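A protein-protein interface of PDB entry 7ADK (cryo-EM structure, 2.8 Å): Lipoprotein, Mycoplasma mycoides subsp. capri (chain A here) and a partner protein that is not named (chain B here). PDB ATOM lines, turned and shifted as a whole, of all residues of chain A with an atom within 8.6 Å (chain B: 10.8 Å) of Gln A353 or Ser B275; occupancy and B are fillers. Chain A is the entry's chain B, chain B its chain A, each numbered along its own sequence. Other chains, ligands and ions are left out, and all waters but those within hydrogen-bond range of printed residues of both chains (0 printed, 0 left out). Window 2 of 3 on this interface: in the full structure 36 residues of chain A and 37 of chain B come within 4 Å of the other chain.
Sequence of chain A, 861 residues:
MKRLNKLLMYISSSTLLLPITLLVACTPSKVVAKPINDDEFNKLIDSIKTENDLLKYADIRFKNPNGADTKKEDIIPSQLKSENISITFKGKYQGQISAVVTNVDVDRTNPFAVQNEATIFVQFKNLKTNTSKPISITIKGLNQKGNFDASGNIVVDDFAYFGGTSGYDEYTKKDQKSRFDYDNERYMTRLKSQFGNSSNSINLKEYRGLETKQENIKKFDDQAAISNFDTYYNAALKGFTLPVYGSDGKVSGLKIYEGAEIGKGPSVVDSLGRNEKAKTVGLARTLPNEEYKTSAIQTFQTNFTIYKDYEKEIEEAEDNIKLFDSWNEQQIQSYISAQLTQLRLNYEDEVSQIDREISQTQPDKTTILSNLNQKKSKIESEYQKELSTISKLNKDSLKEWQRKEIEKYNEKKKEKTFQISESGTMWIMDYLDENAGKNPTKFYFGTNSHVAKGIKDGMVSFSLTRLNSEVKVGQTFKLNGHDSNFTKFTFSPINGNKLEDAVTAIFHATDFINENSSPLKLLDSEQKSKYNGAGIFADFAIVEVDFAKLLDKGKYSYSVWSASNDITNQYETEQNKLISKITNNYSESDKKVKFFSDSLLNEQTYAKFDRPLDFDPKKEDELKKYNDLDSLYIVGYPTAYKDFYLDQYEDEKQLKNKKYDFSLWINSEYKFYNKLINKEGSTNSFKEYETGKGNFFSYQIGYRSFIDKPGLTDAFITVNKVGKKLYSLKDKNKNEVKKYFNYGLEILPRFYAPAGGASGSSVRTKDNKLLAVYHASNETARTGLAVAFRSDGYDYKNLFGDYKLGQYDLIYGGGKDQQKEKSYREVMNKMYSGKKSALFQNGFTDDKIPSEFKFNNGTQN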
ATOM      1  N   ASN A 346     -12.400  18.743   3.164  1.00  0.00           N
ATOM      2  CA  ASN A 346     -12.549  20.079   2.576  1.00  0.00           C
ATOM      3  C   ASN A 346     -13.250  21.119   3.496  1.00  0.00           C
ATOM      4  O   ASN A 346     -13.496  22.234   3.038  1.00  0.00           O
ATOM      5  CB  ASN A 346     -13.232  19.958   1.191  1.00  0.00           C
ATOM      6  CG  ASN A 346     -12.418  19.253   0.110  1.00  0.00           C
ATOM      7  OD1 ASN A 346     -11.206  19.184   0.137  1.00  0.00           O
ATOM      8  ND2 ASN A 346     -13.038  18.755  -0.921  1.00  0.00           N
ATOM      9  N   GLU A 348     -12.320  22.837   6.523  1.00  0.00           N
ATOM     10  CA  GLU A 348     -11.474  23.837   7.222  1.00  0.00           C
ATOM     11  C   GLU A 348     -10.372  24.487   6.340  1.00  0.00           C
ATOM     12  O   GLU A 348      -9.254  24.744   6.799  1.00  0.00           O
ATOM     13  CB  GLU A 348     -10.891  23.220   8.509  1.00  0.00           C
ATOM     14  CG  GLU A 348     -11.909  22.681   9.527  1.00  0.00           C
ATOM     15  CD  GLU A 348     -12.629  23.771  10.332  1.00  0.00           C
ATOM     16  OE1 GLU A 348     -13.030  23.492  11.474  1.00  0.00           O
ATOM     17  OE2 GLU A 348     -12.804  24.913   9.869  1.00  0.00           O
ATOM     18  N   ASP A 349     -10.633  24.704   5.043  1.00  0.00           N
ATOM     19  CA  ASP A 349      -9.648  25.163   4.042  1.00  0.00           C
ATOM     20  C   ASP A 349     -10.040  26.466   3.319  1.00  0.00           C
ATOM     21  O   ASP A 349      -9.975  26.581   2.101  1.00  0.00           O
ATOM     22  CB  ASP A 349      -9.311  24.030   3.068  1.00  0.00           C
ATOM     23  CG  ASP A 349      -8.549  22.864   3.676  1.00  0.00           C
ATOM     24  OD1 ASP A 349      -7.696  23.071   4.560  1.00  0.00           O
ATOM     25  OD2 ASP A 349      -8.741  21.732   3.197  1.00  0.00           O
ATOM     26  N   GLU A 350     -10.442  27.481   4.078  1.00  0.00           N
ATOM     27  CA  GLU A 350     -10.815  28.819   3.601  1.00  0.00           C
ATOM     28  C   GLU A 350      -9.651  29.647   2.997  1.00  0.00           C
ATOM     29  O   GLU A 350      -9.919  30.570   2.237  1.00  0.00           O
ATOM     30  CB  GLU A 350     -11.552  29.585   4.720  1.00  0.00           C
ATOM     31  CG  GLU A 350     -10.776  29.857   6.024  1.00  0.00           C
ATOM     32  CD  GLU A 350     -10.914  28.781   7.121  1.00  0.00           C
ATOM     33  OE1 GLU A 350     -11.131  27.590   6.812  1.00  0.00           O
ATOM     34  OE2 GLU A 350     -10.778  29.121   8.317  1.00  0.00           O
ATOM     35  N   VAL A 351      -8.407  29.326   3.342  1.00  0.00           N
ATOM     36  CA  VAL A 351      -7.185  30.011   2.890  1.00  0.00           C
ATOM     37  C   VAL A 351      -6.134  29.002   2.440  1.00  0.00           C
ATOM     38  O   VAL A 351      -5.506  29.171   1.396  1.00  0.00           O
ATOM     39  CB  VAL A 351      -6.628  30.928   4.001  1.00  0.00           C
ATOM     40  CG1 VAL A 351      -5.292  31.558   3.638  1.00  0.00           C
ATOM     41  CG2 VAL A 351      -7.603  32.060   4.321  1.00  0.00           C
ATOM     42  N   SER A 352      -5.957  27.927   3.209  1.00  0.00           N
ATOM     43  CA  SER A 352      -4.977  26.871   2.947  1.00  0.00           C
ATOM     44  C   SER A 352      -5.174  26.232   1.569  1.00  0.00           C
ATOM     45  O   SER A 352      -6.289  25.879   1.186  1.00  0.00           O
ATOM     46  CB  SER A 352      -5.063  25.807   4.045  1.00  0.00           C
ATOM     47  OG  SER A 352      -4.974  26.396   5.317  1.00  0.00           O
ATOM     48  N   GLN A 353      -4.085  26.073   0.817  1.00  0.00           N
ATOM     49  CA  GLN A 353      -4.112  25.545  -0.547  1.00  0.00           C
ATOM     50  C   GLN A 353      -4.669  24.116  -0.590  1.00  0.00           C
ATOM     51  O   GLN A 353      -4.376  23.295   0.285  1.00  0.00           O
ATOM     52  CB  GLN A 353      -2.718  25.645  -1.192  1.00  0.00           C
ATOM     53  CG  GLN A 353      -1.684  24.609  -0.702  1.00  0.00           C
ATOM     54  CD  GLN A 353      -0.259  24.881  -1.163  1.00  0.00           C
ATOM     55  OE1 GLN A 353       0.119  25.984  -1.519  1.00  0.00           O
ATOM     56  NE2 GLN A 353       0.604  23.899  -1.160  1.00  0.00           N
ATOM     57  N   ILE A 354      -5.511  23.844  -1.594  1.00  0.00           N
ATOM     58  CA  ILE A 354      -6.177  22.548  -1.757  1.00  0.00           C
ATOM     59  C   ILE A 354      -5.277  21.613  -2.562  1.00  0.00           C
ATOM     60  O   ILE A 354      -5.522  21.276  -3.716  1.00  0.00           O
ATOM     61  CB  ILE A 354      -7.619  22.643  -2.311  1.00  0.00           C
ATOM     62  CG1 ILE A 354      -8.454  23.836  -1.812  1.00  0.00           C
ATOM     63  CG2 ILE A 354      -8.340  21.320  -1.983  1.00  0.00           C
ATOM     64  CD1 ILE A 354      -8.728  23.843  -0.312  1.00  0.00           C
ATOM     65  N   ASP A 355      -4.202  21.168  -1.923  1.00  0.00           N
ATOM     66  CA  ASP A 355      -3.338  20.099  -2.442  1.00  0.00           C
ATOM     67  C   ASP A 355      -4.148  18.809  -2.710  1.00  0.00           C
ATOM     68  O   ASP A 355      -3.871  18.023  -3.608  1.00  0.00           O
ATOM     69  CB  ASP A 355      -2.248  19.874  -1.392  1.00  0.00           C
ATOM     70  CG  ASP A 355      -1.075  19.022  -1.870  1.00  0.00           C
ATOM     71  OD1 ASP A 355      -0.857  18.880  -3.091  1.00  0.00           O
ATOM     72  OD2 ASP A 355      -0.328  18.520  -1.004  1.00  0.00           O
ATOM     73  N   ARG A 356      -5.232  18.645  -1.946  1.00  0.00           N
ATOM     74  CA  ARG A 356      -6.168  17.524  -1.961  1.00  0.00           C
ATOM     75  C   ARG A 356      -6.902  17.316  -3.283  1.00  0.00           C
ATOM     76  O   ARG A 356      -7.343  16.200  -3.530  1.00  0.00           O
ATOM     77  CB  ARG A 356      -7.153  17.747  -0.811  1.00  0.00           C
ATOM     78  CG  ARG A 356      -7.793  16.442  -0.319  1.00  0.00           C
ATOM     79  CD  ARG A 356      -8.706  16.650   0.895  1.00  0.00           C
ATOM     80  NE  ARG A 356      -8.011  17.351   1.987  1.00  0.00           N
ATOM     81  CZ  ARG A 356      -8.119  18.623   2.312  1.00  0.00           C
ATOM     82  NH1 ARG A 356      -8.918  19.450   1.721  1.00  0.00           N
ATOM     83  NH2 ARG A 356      -7.402  19.126   3.260  1.00  0.00           N
ATOM     84  N   GLU A 357      -7.000  18.319  -4.157  1.00  0.00           N
ATOM     85  CA  GLU A 357      -7.624  18.145  -5.479  1.00  0.00           C
ATOM     86  C   GLU A 357      -6.915  17.067  -6.318  1.00  0.00           C
ATOM     87  O   GLU A 357      -7.544  16.400  -7.133  1.00  0.00           O
ATOM     88  CB  GLU A 357      -7.636  19.458  -6.278  1.00  0.00           C
ATOM     89  CG  GLU A 357      -8.362  20.650  -5.637  1.00  0.00           C
ATOM     90  CD  GLU A 357      -9.859  20.468  -5.367  1.00  0.00           C
ATOM     91  OE1 GLU A 357     -10.442  19.479  -5.765  1.00  0.00           O
ATOM     92  OE2 GLU A 357     -10.479  21.354  -4.768  1.00  0.00           O
ATOM     93  N   LEU B 224      12.380  24.748   6.014  1.00  0.00           N
ATOM     94  CA  LEU B 224      11.074  24.599   6.684  1.00  0.00           C
ATOM     95  C   LEU B 224      10.284  23.340   6.280  1.00  0.00           C
ATOM     96  O   LEU B 224       9.535  22.792   7.084  1.00  0.00           O
ATOM     97  CB  LEU B 224      10.271  25.890   6.440  1.00  0.00           C
ATOM     98  CG  LEU B 224       8.982  25.994   7.279  1.00  0.00           C
ATOM     99  CD1 LEU B 224       8.775  27.420   7.766  1.00  0.00           C
ATOM    100  CD2 LEU B 224       7.744  25.610   6.472  1.00  0.00           C
ATOM    101  N   ASN B 225      10.472  22.840   5.058  1.00  0.00           N
ATOM    102  CA  ASN B 225       9.789  21.654   4.545  1.00  0.00           C
ATOM    103  C   ASN B 225      10.255  20.329   5.187  1.00  0.00           C
ATOM    104  O   ASN B 225       9.726  19.275   4.846  1.00  0.00           O
ATOM    105  CB  ASN B 225       9.867  21.629   3.013  1.00  0.00           C
ATOM    106  CG  ASN B 225       9.462  22.958   2.409  1.00  0.00           C
ATOM    107  OD1 ASN B 225      10.294  23.813   2.152  1.00  0.00           O
ATOM    108  ND2 ASN B 225       8.191  23.201   2.232  1.00  0.00           N
ATOM    109  N   LYS B 268       4.821  36.778  13.023  1.00  0.00           N
ATOM    110  CA  LYS B 268       5.129  37.444  11.751  1.00  0.00           C
ATOM    111  C   LYS B 268       5.047  36.480  10.564  1.00  0.00           C
ATOM    112  O   LYS B 268       4.608  36.866   9.489  1.00  0.00           O
ATOM    113  CB  LYS B 268       6.492  38.151  11.830  1.00  0.00           C
ATOM    114  CG  LYS B 268       6.427  39.418  12.697  1.00  0.00           C
ATOM    115  CD  LYS B 268       7.647  40.332  12.544  1.00  0.00           C
ATOM    116  CE  LYS B 268       8.943  39.778  13.137  1.00  0.00           C
ATOM    117  NZ  LYS B 268       9.011  39.957  14.603  1.00  0.00           N
ATOM    118  N   GLU B 269       5.476  35.229  10.723  1.00  0.00           N
ATOM    119  CA  GLU B 269       5.454  34.229   9.641  1.00  0.00           C
ATOM    120  C   GLU B 269       4.059  33.627   9.395  1.00  0.00           C
ATOM    121  O   GLU B 269       3.704  33.349   8.253  1.00  0.00           O
ATOM    122  CB  GLU B 269       6.461  33.106   9.938  1.00  0.00           C
ATOM    123  CG  GLU B 269       7.925  33.546   9.805  1.00  0.00           C
ATOM    124  CD  GLU B 269       8.888  32.355   9.756  1.00  0.00           C
ATOM    125  OE1 GLU B 269       8.810  31.461  10.623  1.00  0.00           O
ATOM    126  OE2 GLU B 269       9.755  32.301   8.863  1.00  0.00           O
ATOM    127  N   TYR B 270       3.258  33.433  10.445  1.00  0.00           N
ATOM    128  CA  TYR B 270       1.982  32.716  10.408  1.00  0.00           C
ATOM    129  C   TYR B 270       0.970  33.208   9.359  1.00  0.00           C
ATOM    130  O   TYR B 270       0.506  32.370   8.585  1.00  0.00           O
ATOM    131  CB  TYR B 270       1.382  32.676  11.821  1.00  0.00           C
ATOM    132  CG  TYR B 270      -0.070  32.233  11.887  1.00  0.00           C
ATOM    133  CD1 TYR B 270      -0.425  30.874  11.955  1.00  0.00           C
ATOM    134  CD2 TYR B 270      -1.087  33.203  11.862  1.00  0.00           C
ATOM    135  CE1 TYR B 270      -1.777  30.490  11.984  1.00  0.00           C
ATOM    136  CE2 TYR B 270      -2.436  32.828  11.882  1.00  0.00           C
ATOM    137  CZ  TYR B 270      -2.788  31.468  11.943  1.00  0.00           C
ATOM    138  OH  TYR B 270      -4.090  31.107  11.978  1.00  0.00           O
ATOM    139  N   PRO B 271       0.632  34.509   9.263  1.00  0.00           N
ATOM    140  CA  PRO B 271      -0.445  34.977   8.391  1.00  0.00           C
ATOM    141  C   PRO B 271      -0.159  34.796   6.894  1.00  0.00           C
ATOM    142  O   PRO B 271      -1.097  34.650   6.104  1.00  0.00           O
ATOM    143  CB  PRO B 271      -0.675  36.439   8.769  1.00  0.00           C
ATOM    144  CG  PRO B 271       0.629  36.883   9.401  1.00  0.00           C
ATOM    145  CD  PRO B 271       1.140  35.614  10.057  1.00  0.00           C
ATOM    146  N   LYS B 272       1.121  34.749   6.501  1.00  0.00           N
ATOM    147  CA  LYS B 272       1.538  34.405   5.136  1.00  0.00           C
ATOM    148  C   LYS B 272       1.629  32.893   4.972  1.00  0.00           C
ATOM    149  O   LYS B 272       0.980  32.322   4.097  1.00  0.00           O
ATOM    150  CB  LYS B 272       2.861  35.109   4.783  1.00  0.00           C
ATOM    151  CG  LYS B 272       2.792  36.645   4.822  1.00  0.00           C
ATOM    152  CD  LYS B 272       1.738  37.251   3.892  1.00  0.00           C
ATOM    153  CE  LYS B 272       1.819  38.774   3.813  1.00  0.00           C
ATOM    154  NZ  LYS B 272       1.465  39.436   5.080  1.00  0.00           N
ATOM    155  N   LEU B 273       2.398  32.239   5.849  1.00  0.00           N
ATOM    156  CA  LEU B 273       2.747  30.818   5.752  1.00  0.00           C
ATOM    157  C   LEU B 273       1.528  29.891   5.872  1.00  0.00           C
ATOM    158  O   LEU B 273       1.550  28.814   5.289  1.00  0.00           O
ATOM    159  CB  LEU B 273       3.821  30.502   6.811  1.00  0.00           C
ATOM    160  CG  LEU B 273       4.534  29.149   6.634  1.00  0.00           C
ATOM    161  CD1 LEU B 273       5.624  29.194   5.572  1.00  0.00           C
ATOM    162  CD2 LEU B 273       5.200  28.752   7.937  1.00  0.00           C
ATOM    163  N   LYS B 274       0.445  30.320   6.535  1.00  0.00           N
ATOM    164  CA  LYS B 274      -0.841  29.605   6.637  1.00  0.00           C
ATOM    165  C   LYS B 274      -1.362  29.069   5.301  1.00  0.00           C
ATOM    166  O   LYS B 274      -1.887  27.962   5.244  1.00  0.00           O
ATOM    167  CB  LYS B 274      -1.850  30.575   7.283  1.00  0.00           C
ATOM    168  CG  LYS B 274      -3.306  30.092   7.325  1.00  0.00           C
ATOM    169  CD  LYS B 274      -3.507  28.837   8.183  1.00  0.00           C
ATOM    170  CE  LYS B 274      -4.782  28.074   7.855  1.00  0.00           C
ATOM    171  NZ  LYS B 274      -5.995  28.858   8.082  1.00  0.00           N
ATOM    172  N   SER B 275      -1.183  29.829   4.225  1.00  0.00           N
ATOM    173  CA  SER B 275      -1.549  29.445   2.851  1.00  0.00           C
ATOM    174  C   SER B 275      -0.650  28.372   2.204  1.00  0.00           C
ATOM    175  O   SER B 275      -1.006  27.818   1.174  1.00  0.00           O
ATOM    176  CB  SER B 275      -1.575  30.703   1.979  1.00  0.00           C
ATOM    177  OG  SER B 275      -0.284  31.253   1.796  1.00  0.00           O
ATOM    178  N   LYS B 276       0.515  28.071   2.789  1.00  0.00           N
ATOM    179  CA  LYS B 276       1.615  27.322   2.158  1.00  0.00           C
ATOM    180  C   LYS B 276       1.822  25.911   2.733  1.00  0.00           C
ATOM    181  O   LYS B 276       2.899  25.341   2.565  1.00  0.00           O
ATOM    182  CB  LYS B 276       2.910  28.163   2.193  1.00  0.00           C
ATOM    183  CG  LYS B 276       2.803  29.636   1.742  1.00  0.00           C
ATOM    184  CD  LYS B 276       2.240  29.855   0.327  1.00  0.00           C
ATOM    185  CE  LYS B 276       3.151  29.391  -0.813  1.00  0.00           C
ATOM    186  NZ  LYS B 276       4.217  30.360  -1.120  1.00  0.00           N
ATOM    187  N   PHE B 277       0.817  25.324   3.388  1.00  0.00           N
ATOM    188  CA  PHE B 277       0.880  23.959   3.932  1.00  0.00           C
ATOM    189  C   PHE B 277       0.077  22.943   3.114  1.00  0.00           C
ATOM    190  O   PHE B 277      -1.042  23.197   2.672  1.00  0.00           O
ATOM    191  CB  PHE B 277       0.472  23.933   5.405  1.00  0.00           C
ATOM    192  CG  PHE B 277       1.541  24.478   6.318  1.00  0.00           C
ATOM    193  CD1 PHE B 277       2.725  23.746   6.515  1.00  0.00           C
ATOM    194  CD2 PHE B 277       1.368  25.709   6.967  1.00  0.00           C
ATOM    195  CE1 PHE B 277       3.729  24.239   7.362  1.00  0.00           C
ATOM    196  CE2 PHE B 277       2.368  26.194   7.826  1.00  0.00           C
ATOM    197  CZ  PHE B 277       3.547  25.461   8.023  1.00  0.00           C
ATOM    198  N   GLN B 278       0.676  21.767   2.923  1.00  0.00           N
ATOM    199  CA  GLN B 278       0.165  20.704   2.039  1.00  0.00           C
ATOM    200  C   GLN B 278      -0.878  19.762   2.675  1.00  0.00           C
ATOM    201  O   GLN B 278      -1.542  19.010   1.961  1.00  0.00           O
ATOM    202  CB  GLN B 278       1.346  19.870   1.509  1.00  0.00           C
ATOM    203  CG  GLN B 278       2.227  20.606   0.487  1.00  0.00           C
ATOM    204  CD  GLN B 278       3.001  21.783   1.068  1.00  0.00           C
ATOM    205  OE1 GLN B 278       3.607  21.700   2.125  1.00  0.00           O
ATOM    206  NE2 GLN B 278       2.978  22.930   0.445  1.00  0.00           N
ATOM    207  N   THR B 279      -1.006  19.749   4.002  1.00  0.00           N
ATOM    208  CA  THR B 279      -1.877  18.840   4.766  1.00  0.00           C
ATOM    209  C   THR B 279      -2.256  19.530   6.070  1.00  0.00           C
ATOM    210  O   THR B 279      -1.426  20.258   6.606  1.00  0.00           O
ATOM    211  CB  THR B 279      -1.140  17.528   5.104  1.00  0.00           C
ATOM    212  OG1 THR B 279      -0.500  16.938   3.997  1.00  0.00           O
ATOM    213  CG2 THR B 279      -2.025  16.443   5.692  1.00  0.00           C
ATOM    214  N   LYS B 280      -3.431  19.261   6.655  1.00  0.00           N
ATOM    215  CA  LYS B 280      -3.820  19.877   7.936  1.00  0.00           C
ATOM    216  C   LYS B 280      -2.840  19.580   9.057  1.00  0.00           C
ATOM    217  O   LYS B 280      -2.372  20.506   9.695  1.00  0.00           O
ATOM    218  CB  LYS B 280      -5.256  19.494   8.319  1.00  0.00           C
ATOM    219  CG  LYS B 280      -6.340  20.113   7.428  1.00  0.00           C
ATOM    220  CD  LYS B 280      -6.368  21.653   7.436  1.00  0.00           C
ATOM    221  CE  LYS B 280      -5.506  22.293   6.344  1.00  0.00           C
ATOM    222  NZ  LYS B 280      -5.546  23.754   6.390  1.00  0.00           N
ATOM    223  N   ASN B 281      -2.428  18.320   9.241  1.00  0.00           N
ATOM    224  CA  ASN B 281      -1.432  17.928  10.256  1.00  0.00           C
ATOM    225  C   ASN B 281      -0.085  18.652  10.087  1.00  0.00           C
ATOM    226  O   ASN B 281       0.443  19.140  11.076  1.00  0.00           O
ATOM    227  CB  ASN B 281      -1.245  16.396  10.285  1.00  0.00           C
ATOM    228  CG  ASN B 281      -2.365  15.636  10.988  1.00  0.00           C
ATOM    229  OD1 ASN B 281      -3.021  16.122  11.892  1.00  0.00           O
ATOM    230  ND2 ASN B 281      -2.620  14.411  10.604  1.00  0.00           N
ATOM    231  N   GLN B 282       0.449  18.775   8.866  1.00  0.00           N
ATOM    232  CA  GLN B 282       1.680  19.539   8.587  1.00  0.00           C
ATOM    233  C   GLN B 282       1.568  21.009   9.017  1.00  0.00           C
ATOM    234  O   GLN B 282       2.514  21.545   9.577  1.00  0.00           O
ATOM    235  CB  GLN B 282       2.033  19.471   7.091  1.00  0.00           C
ATOM    236  CG  GLN B 282       2.452  18.064   6.671  1.00  0.00           C
ATOM    237  CD  GLN B 282       3.040  18.000   5.263  1.00  0.00           C
ATOM    238  OE1 GLN B 282       4.135  18.469   5.001  1.00  0.00           O
ATOM    239  NE2 GLN B 282       2.380  17.403   4.298  1.00  0.00           N
ATOM    240  N   GLU B 283       0.412  21.639   8.811  1.00  0.00           N
ATOM    241  CA  GLU B 283       0.066  22.911   9.448  1.00  0.00           C
ATOM    242  C   GLU B 283       0.102  22.838  10.976  1.00  0.00           C
ATOM    243  O   GLU B 283       0.911  23.518  11.599  1.00  0.00           O
ATOM    244  CB  GLU B 283      -1.267  23.435   8.873  1.00  0.00           C
ATOM    245  CG  GLU B 283      -2.041  24.529   9.630  1.00  0.00           C
ATOM    246  CD  GLU B 283      -1.349  25.867   9.915  1.00  0.00           C
ATOM    247  OE1 GLU B 283      -0.113  25.998   9.811  1.00  0.00           O
ATOM    248  OE2 GLU B 283      -2.086  26.809  10.280  1.00  0.00           O
ATOM    249  N   TYR B 284      -0.745  22.055  11.642  1.00  0.00           N
ATOM    250  CA  TYR B 284      -0.990  22.358  13.054  1.00  0.00           C
ATOM    251  C   TYR B 284       0.084  21.739  13.980  1.00  0.00           C
ATOM    252  O   TYR B 284       0.290  22.223  15.088  1.00  0.00           O
ATOM    253  CB  TYR B 284      -2.512  22.325  13.311  1.00  0.00           C
ATOM    254  CG  TYR B 284      -3.322  21.080  13.616  1.00  0.00           C
ATOM    255  CD1 TYR B 284      -3.518  20.111  12.626  1.00  0.00           C
ATOM    256  CD2 TYR B 284      -4.385  21.251  14.522  1.00  0.00           C
ATOM    257  CE1 TYR B 284      -4.587  19.199  12.648  1.00  0.00           C
ATOM    258  CE2 TYR B 284      -5.494  20.392  14.541  1.00  0.00           C
ATOM    259  CZ  TYR B 284      -5.586  19.334  13.622  1.00  0.00           C
ATOM    260  OH  TYR B 284      -6.649  18.497  13.641  1.00  0.00           O
ATOM    261  N   TRP B 286       3.112  22.759  13.106  1.00  0.00           N
ATOM    262  CA  TRP B 286       3.853  24.014  13.124  1.00  0.00           C
ATOM    263  C   TRP B 286       3.279  25.009  14.141  1.00  0.00           C
ATOM    264  O   TRP B 286       3.976  25.945  14.526  1.00  0.00           O
ATOM    265  CB  TRP B 286       3.957  24.572  11.692  1.00  0.00           C
ATOM    266  CG  TRP B 286       4.837  25.762  11.478  1.00  0.00           C
ATOM    267  CD1 TRP B 286       6.169  25.747  11.270  1.00  0.00           C
ATOM    268  CD2 TRP B 286       4.455  27.165  11.425  1.00  0.00           C
ATOM    269  NE1 TRP B 286       6.644  27.038  11.215  1.00  0.00           N
ATOM    270  CE2 TRP B 286       5.634  27.953  11.352  1.00  0.00           C
ATOM    271  CE3 TRP B 286       3.228  27.853  11.399  1.00  0.00           C
ATOM    272  CZ2 TRP B 286       5.602  29.351  11.376  1.00  0.00           C
ATOM    273  CZ3 TRP B 286       3.185  29.256  11.335  1.00  0.00           C
ATOM    274  CH2 TRP B 286       4.365  30.007  11.371  1.00  0.00           C
ATOM    275  N   LEU B 287       2.054  24.841  14.648  1.00  0.00           N
ATOM    276  CA  LEU B 287       1.563  25.628  15.790  1.00  0.00           C
ATOM    277  C   LEU B 287       2.209  25.146  17.092  1.00  0.00           C
ATOM    278  O   LEU B 287       2.925  25.910  17.716  1.00  0.00           O
ATOM    279  CB  LEU B 287       0.025  25.653  15.884  1.00  0.00           C
ATOM    280  CG  LEU B 287      -0.764  26.628  15.003  1.00  0.00           C
ATOM    281  CD1 LEU B 287      -0.245  28.045  15.113  1.00  0.00           C
ATOM    282  CD2 LEU B 287      -0.791  26.251  13.545  1.00  0.00           C
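Of the 21 printed residues of chain B, 5 touch a printed residue of chain A.
Of the 11 printed residues of chain A, 5 touch a printed residue of chain B.
Printed residues of chain A that touch a printed residue of chain B: Glu A348, Asp A349, Ser A352, Gln A353 and Asp A355.
Among the printed residues, 8 pairs touch across the chains.
Among the printed residues, Asp or Glu carboxylates within 4 Å of a Lys or Arg side-chain nitrogen of the other chain: Asp A349 with Lys B280.
Lys B280 touches Glu A348 (NZ to O, 3.9 Å).
O of Phe B277 touches CG of Gln A353, at 3.7 Å.
Gln A353 touches just these residues of chain B: Ser B275 (3.4 Å), Phe B277 (3.7 Å) and Gln B278 (3.0 Å).
Ser B275 touches one residue of chain A.
No residue of chain B comes within 4 Å of Val A351.
Of the printed residues of chain A, Phe B277 touches Gln A353.
Of the printed residues of chain B, Glu A348 touches Lys B280 (3.9 Å).
Lys B272 touches none of the printed residues of chain A.
The nearest residue of chain A that does not touch Ser B275 is Val A351 (4.2 Å).
O of Lys B274 lies close to OG of Ser A352 (3.5 Å).
The backbone carbonyl oxygen (O) of Ser B275 sits close to the side-chain amide oxygen (OE1) of Gln A353 (3.4 Å).
NE2 of Gln B278 lies close to NE2 of Gln A353, at 3.0 Å.
NZ of Lys B280 lies within salt-bridge range of OD1 of Asp A349.
NZ of Lys B280 sits at hydrogen-bond distance from OG of Ser A352.
O of Gln B278 sits close to OD2 of Asp A355, at 3.2 Å.
The backbone carbonyl oxygen of Lys B272 is in hydrogen-bond range of the side-chain hydroxyl of Ser B275.
The side-chain amide nitrogen (NE2) of Gln B278 sits at hydrogen-bond distance from the backbone carbonyl oxygen (O) of Lys B276 (3.2 Å).
The side-chain carboxylate (OD2) of Asp A349 lies within salt-bridge range of the guanidinium group (NH1) of Arg A356 (2.7 Å).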
